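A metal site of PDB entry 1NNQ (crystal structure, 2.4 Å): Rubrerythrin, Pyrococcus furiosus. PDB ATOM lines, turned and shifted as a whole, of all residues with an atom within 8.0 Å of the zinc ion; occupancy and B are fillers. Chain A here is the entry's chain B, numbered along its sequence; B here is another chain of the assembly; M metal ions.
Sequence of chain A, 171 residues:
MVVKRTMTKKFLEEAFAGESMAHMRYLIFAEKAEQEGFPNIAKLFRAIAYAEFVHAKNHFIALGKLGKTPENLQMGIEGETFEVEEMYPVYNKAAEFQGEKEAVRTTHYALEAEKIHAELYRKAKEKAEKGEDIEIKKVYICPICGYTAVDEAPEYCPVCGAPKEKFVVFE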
ATOM      1  N   TYR A 109     -22.009  28.371  14.774  1.00  0.00           N
ATOM      2  CA  TYR A 109     -21.224  28.253  15.974  1.00  0.00           C
ATOM      3  C   TYR A 109     -22.106  27.731  17.139  1.00  0.00           C
ATOM      4  O   TYR A 109     -21.780  26.731  17.780  1.00  0.00           O
ATOM      5  CB  TYR A 109     -20.634  29.622  16.297  1.00  0.00           C
ATOM      6  CG  TYR A 109     -19.366  29.990  15.529  1.00  0.00           C
ATOM      7  CD1 TYR A 109     -18.793  29.124  14.583  1.00  0.00           C
ATOM      8  CD2 TYR A 109     -18.729  31.223  15.761  1.00  0.00           C
ATOM      9  CE1 TYR A 109     -17.596  29.469  13.888  1.00  0.00           C
ATOM     10  CE2 TYR A 109     -17.545  31.579  15.080  1.00  0.00           C
ATOM     11  CZ  TYR A 109     -16.981  30.700  14.150  1.00  0.00           C
ATOM     12  OH  TYR A 109     -15.811  31.035  13.488  1.00  0.00           O
ATOM     13  N   ILE A 141     -13.695  24.903  26.876  1.00  0.00           N
ATOM     14  CA  ILE A 141     -14.573  25.719  26.032  1.00  0.00           C
ATOM     15  C   ILE A 141     -13.800  26.603  25.056  1.00  0.00           C
ATOM     16  O   ILE A 141     -12.929  27.384  25.471  1.00  0.00           O
ATOM     17  CB  ILE A 141     -15.542  26.651  26.902  1.00  0.00           C
ATOM     18  CG1 ILE A 141     -16.241  25.881  28.038  1.00  0.00           C
ATOM     19  CG2 ILE A 141     -16.542  27.430  26.008  1.00  0.00           C
ATOM     20  CD1 ILE A 141     -17.138  24.729  27.620  1.00  0.00           C
ATOM     21  N   CYS A 142     -14.138  26.502  23.771  1.00  0.00           N
ATOM     22  CA  CYS A 142     -13.596  27.419  22.782  1.00  0.00           C
ATOM     23  C   CYS A 142     -14.121  28.833  23.008  1.00  0.00           C
ATOM     24  O   CYS A 142     -15.343  29.071  22.990  1.00  0.00           O
ATOM     25  CB  CYS A 142     -13.874  26.938  21.361  1.00  0.00           C
ATOM     26  SG  CYS A 142     -13.119  27.998  20.081  1.00  0.00           S
ATOM     27  N   PRO A 143     -13.195  29.781  23.202  1.00  0.00           N
ATOM     28  CA  PRO A 143     -13.557  31.190  23.407  1.00  0.00           C
ATOM     29  C   PRO A 143     -14.050  31.891  22.153  1.00  0.00           C
ATOM     30  O   PRO A 143     -14.460  33.023  22.279  1.00  0.00           O
ATOM     31  CB  PRO A 143     -12.239  31.837  23.868  1.00  0.00           C
ATOM     32  CG  PRO A 143     -11.173  30.966  23.285  1.00  0.00           C
ATOM     33  CD  PRO A 143     -11.731  29.567  23.241  1.00  0.00           C
ATOM     34  N   ILE A 144     -14.025  31.240  20.999  1.00  0.00           N
ATOM     35  CA  ILE A 144     -14.448  31.866  19.745  1.00  0.00           C
ATOM     36  C   ILE A 144     -15.821  31.357  19.314  1.00  0.00           C
ATOM     37  O   ILE A 144     -16.701  32.141  18.940  1.00  0.00           O
ATOM     38  CB  ILE A 144     -13.394  31.592  18.644  1.00  0.00           C
ATOM     39  CG1 ILE A 144     -12.091  32.307  18.995  1.00  0.00           C
ATOM     40  CG2 ILE A 144     -13.892  32.061  17.263  1.00  0.00           C
ATOM     41  CD1 ILE A 144     -10.937  31.538  18.559  1.00  0.00           C
ATOM     42  N   CYS A 145     -16.013  30.046  19.353  1.00  0.00           N
ATOM     43  CA  CYS A 145     -17.274  29.505  18.901  1.00  0.00           C
ATOM     44  C   CYS A 145     -18.102  28.834  20.008  1.00  0.00           C
ATOM     45  O   CYS A 145     -19.232  28.432  19.753  1.00  0.00           O
ATOM     46  CB  CYS A 145     -17.057  28.570  17.727  1.00  0.00           C
ATOM     47  SG  CYS A 145     -16.404  26.963  18.228  1.00  0.00           S
ATOM     48  N   GLY A 146     -17.545  28.680  21.196  1.00  0.00           N
ATOM     49  CA  GLY A 146     -18.244  28.005  22.283  1.00  0.00           C
ATOM     50  C   GLY A 146     -18.217  26.483  22.284  1.00  0.00           C
ATOM     51  O   GLY A 146     -18.878  25.871  23.129  1.00  0.00           O
ATOM     52  N   TYR A 147     -17.479  25.869  21.360  1.00  0.00           N
ATOM     53  CA  TYR A 147     -17.305  24.417  21.343  1.00  0.00           C
ATOM     54  C   TYR A 147     -16.839  23.889  22.686  1.00  0.00           C
ATOM     55  O   TYR A 147     -15.938  24.442  23.343  1.00  0.00           O
ATOM     56  CB  TYR A 147     -16.293  23.988  20.274  1.00  0.00           C
ATOM     57  CG  TYR A 147     -16.228  22.496  20.039  1.00  0.00           C
ATOM     58  CD1 TYR A 147     -17.139  21.877  19.204  1.00  0.00           C
ATOM     59  CD2 TYR A 147     -15.240  21.725  20.646  1.00  0.00           C
ATOM     60  CE1 TYR A 147     -17.077  20.501  18.966  1.00  0.00           C
ATOM     61  CE2 TYR A 147     -15.167  20.340  20.428  1.00  0.00           C
ATOM     62  CZ  TYR A 147     -16.095  19.739  19.591  1.00  0.00           C
ATOM     63  OH  TYR A 147     -16.051  18.367  19.346  1.00  0.00           O
ATOM     64  N   THR A 148     -17.462  22.770  23.049  1.00  0.00           N
ATOM     65  CA  THR A 148     -17.393  22.196  24.384  1.00  0.00           C
ATOM     66  C   THR A 148     -16.800  20.811  24.336  1.00  0.00           C
ATOM     67  O   THR A 148     -17.229  19.973  23.543  1.00  0.00           O
ATOM     68  CB  THR A 148     -18.818  22.148  24.977  1.00  0.00           C
ATOM     69  OG1 THR A 148     -19.391  23.466  24.937  1.00  0.00           O
ATOM     70  CG2 THR A 148     -18.787  21.780  26.474  1.00  0.00           C
ATOM     71  N   TYR A 156      -7.288  20.904  17.614  1.00  0.00           N
ATOM     72  CA  TYR A 156      -7.868  22.177  17.189  1.00  0.00           C
ATOM     73  C   TYR A 156      -9.380  22.091  17.244  1.00  0.00           C
ATOM     74  O   TYR A 156      -9.955  20.993  17.157  1.00  0.00           O
ATOM     75  CB  TYR A 156      -7.432  22.541  15.769  1.00  0.00           C
ATOM     76  CG  TYR A 156      -7.951  21.614  14.683  1.00  0.00           C
ATOM     77  CD1 TYR A 156      -9.126  21.915  13.974  1.00  0.00           C
ATOM     78  CD2 TYR A 156      -7.234  20.453  14.312  1.00  0.00           C
ATOM     79  CE1 TYR A 156      -9.582  21.096  12.966  1.00  0.00           C
ATOM     80  CE2 TYR A 156      -7.695  19.628  13.283  1.00  0.00           C
ATOM     81  CZ  TYR A 156      -8.869  19.958  12.617  1.00  0.00           C
ATOM     82  OH  TYR A 156      -9.337  19.160  11.595  1.00  0.00           O
ATOM     83  N   CYS A 157     -10.033  23.260  17.385  1.00  0.00           N
ATOM     84  CA  CYS A 157     -11.482  23.351  17.343  1.00  0.00           C
ATOM     85  C   CYS A 157     -12.022  22.933  15.978  1.00  0.00           C
ATOM     86  O   CYS A 157     -11.707  23.548  14.975  1.00  0.00           O
ATOM     87  CB  CYS A 157     -11.950  24.757  17.694  1.00  0.00           C
ATOM     88  SG  CYS A 157     -13.755  24.871  17.829  1.00  0.00           S
ATOM     89  N   PRO A 158     -12.817  21.876  15.936  1.00  0.00           N
ATOM     90  CA  PRO A 158     -13.359  21.410  14.652  1.00  0.00           C
ATOM     91  C   PRO A 158     -14.348  22.388  14.042  1.00  0.00           C
ATOM     92  O   PRO A 158     -14.685  22.263  12.874  1.00  0.00           O
ATOM     93  CB  PRO A 158     -14.052  20.086  15.007  1.00  0.00           C
ATOM     94  CG  PRO A 158     -14.357  20.181  16.472  1.00  0.00           C
ATOM     95  CD  PRO A 158     -13.235  21.021  17.067  1.00  0.00           C
ATOM     96  N   VAL A 159     -14.808  23.368  14.811  1.00  0.00           N
ATOM     97  CA  VAL A 159     -15.828  24.293  14.324  1.00  0.00           C
ATOM     98  C   VAL A 159     -15.210  25.557  13.712  1.00  0.00           C
ATOM     99  O   VAL A 159     -15.543  25.937  12.599  1.00  0.00           O
ATOM    100  CB  VAL A 159     -16.872  24.655  15.454  1.00  0.00           C
ATOM    101  CG1 VAL A 159     -17.898  25.699  14.973  1.00  0.00           C
ATOM    102  CG2 VAL A 159     -17.582  23.404  15.975  1.00  0.00           C
ATOM    103  N   CYS A 160     -14.298  26.180  14.440  1.00  0.00           N
ATOM    104  CA  CYS A 160     -13.707  27.455  14.058  1.00  0.00           C
ATOM    105  C   CYS A 160     -12.209  27.348  13.704  1.00  0.00           C
ATOM    106  O   CYS A 160     -11.663  28.271  13.084  1.00  0.00           O
ATOM    107  CB  CYS A 160     -13.946  28.516  15.149  1.00  0.00           C
ATOM    108  SG  CYS A 160     -12.884  28.415  16.628  1.00  0.00           S
ATOM    109  N   GLY A 161     -11.571  26.244  14.093  1.00  0.00           N
ATOM    110  CA  GLY A 161     -10.159  25.992  13.778  1.00  0.00           C
ATOM    111  C   GLY A 161      -9.120  26.429  14.811  1.00  0.00           C
ATOM    112  O   GLY A 161      -7.916  26.318  14.573  1.00  0.00           O
ATOM    113  N   ALA A 162      -9.585  26.948  15.955  1.00  0.00           N
ATOM    114  CA  ALA A 162      -8.707  27.498  16.989  1.00  0.00           C
ATOM    115  C   ALA A 162      -7.815  26.445  17.598  1.00  0.00           C
ATOM    116  O   ALA A 162      -8.248  25.320  17.797  1.00  0.00           O
ATOM    117  CB  ALA A 162      -9.538  28.161  18.082  1.00  0.00           C
ATOM    118  N   PRO A 163      -6.562  26.806  17.908  1.00  0.00           N
ATOM    119  CA  PRO A 163      -5.609  25.867  18.522  1.00  0.00           C
ATOM    120  C   PRO A 163      -6.059  25.376  19.899  1.00  0.00           C
ATOM    121  O   PRO A 163      -6.641  26.159  20.653  1.00  0.00           O
ATOM    122  CB  PRO A 163      -4.323  26.702  18.692  1.00  0.00           C
ATOM    123  CG  PRO A 163      -4.723  28.107  18.529  1.00  0.00           C
ATOM    124  CD  PRO A 163      -5.957  28.127  17.657  1.00  0.00           C
ATOM    125  N   LYS A 166      -5.995  27.780  22.927  1.00  0.00           N
ATOM    126  CA  LYS A 166      -6.915  28.896  23.147  1.00  0.00           C
ATOM    127  C   LYS A 166      -8.090  28.495  24.074  1.00  0.00           C
ATOM    128  O   LYS A 166      -8.719  29.378  24.683  1.00  0.00           O
ATOM    129  CB  LYS A 166      -7.444  29.423  21.822  1.00  0.00           C
ATOM    130  CG  LYS A 166      -7.198  30.918  21.576  1.00  0.00           C
ATOM    131  N   PHE A 167      -8.365  27.187  24.181  1.00  0.00           N
ATOM    132  CA  PHE A 167      -9.482  26.678  24.983  1.00  0.00           C
ATOM    133  C   PHE A 167      -9.399  27.180  26.430  1.00  0.00           C
ATOM    134  O   PHE A 167      -8.305  27.230  27.040  1.00  0.00           O
ATOM    135  CB  PHE A 167      -9.580  25.138  24.922  1.00  0.00           C
ATOM    136  CG  PHE A 167     -10.329  24.592  23.714  1.00  0.00           C
ATOM    137  CD1 PHE A 167     -11.649  24.109  23.842  1.00  0.00           C
ATOM    138  CD2 PHE A 167      -9.714  24.518  22.454  1.00  0.00           C
ATOM    139  CE1 PHE A 167     -12.364  23.569  22.744  1.00  0.00           C
ATOM    140  CE2 PHE A 167     -10.393  23.987  21.327  1.00  0.00           C
ATOM    141  CZ  PHE A 167     -11.727  23.515  21.469  1.00  0.00           C
ATOM    142  N   VAL B  54     -20.297  32.991  25.238  1.00  0.00           N
ATOM    143  CA  VAL B  54     -19.585  33.086  23.954  1.00  0.00           C
ATOM    144  C   VAL B  54     -20.601  33.266  22.841  1.00  0.00           C
ATOM    145  O   VAL B  54     -20.509  34.216  22.044  1.00  0.00           O
ATOM    146  CB  VAL B  54     -18.657  31.848  23.694  1.00  0.00           C
ATOM    147  CG1 VAL B  54     -18.054  31.900  22.273  1.00  0.00           C
ATOM    148  CG2 VAL B  54     -17.509  31.786  24.749  1.00  0.00           C
HETATM  149 ZN    ZN M   1     -14.075  27.172  18.180  1.00  0.00          ZN
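The backbone NH of Cys 142 is in hydrogen-bond range of the backbone carbonyl oxygen of Tyr 147 (2.8 Å).
The side-chain sulfur (SG) of Cys 145 sits close to the backbone NH (N) of Tyr 147, at 3.5 Å.
N of Cys 157 is in hydrogen-bond range of O of Ala 162, at 2.8 Å.
SG of Cys 160 sits close to N of Ala 162.
The backbone NH of Val 159 sits close to the side-chain sulfur of Cys 157 (3.5 Å).
The side-chain sulfur (SG) of Cys 142 sits close to the backbone NH (N) of Ile 144.
The zinc ion is bound by SG of Cys 142 (2.3 Å), SG of Cys 160 (2.3 Å), SG of Cys 145 (2.3 Å) and SG of Cys 157 (2.3 Å).
The zinc ion has four donor atoms within binding distance.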
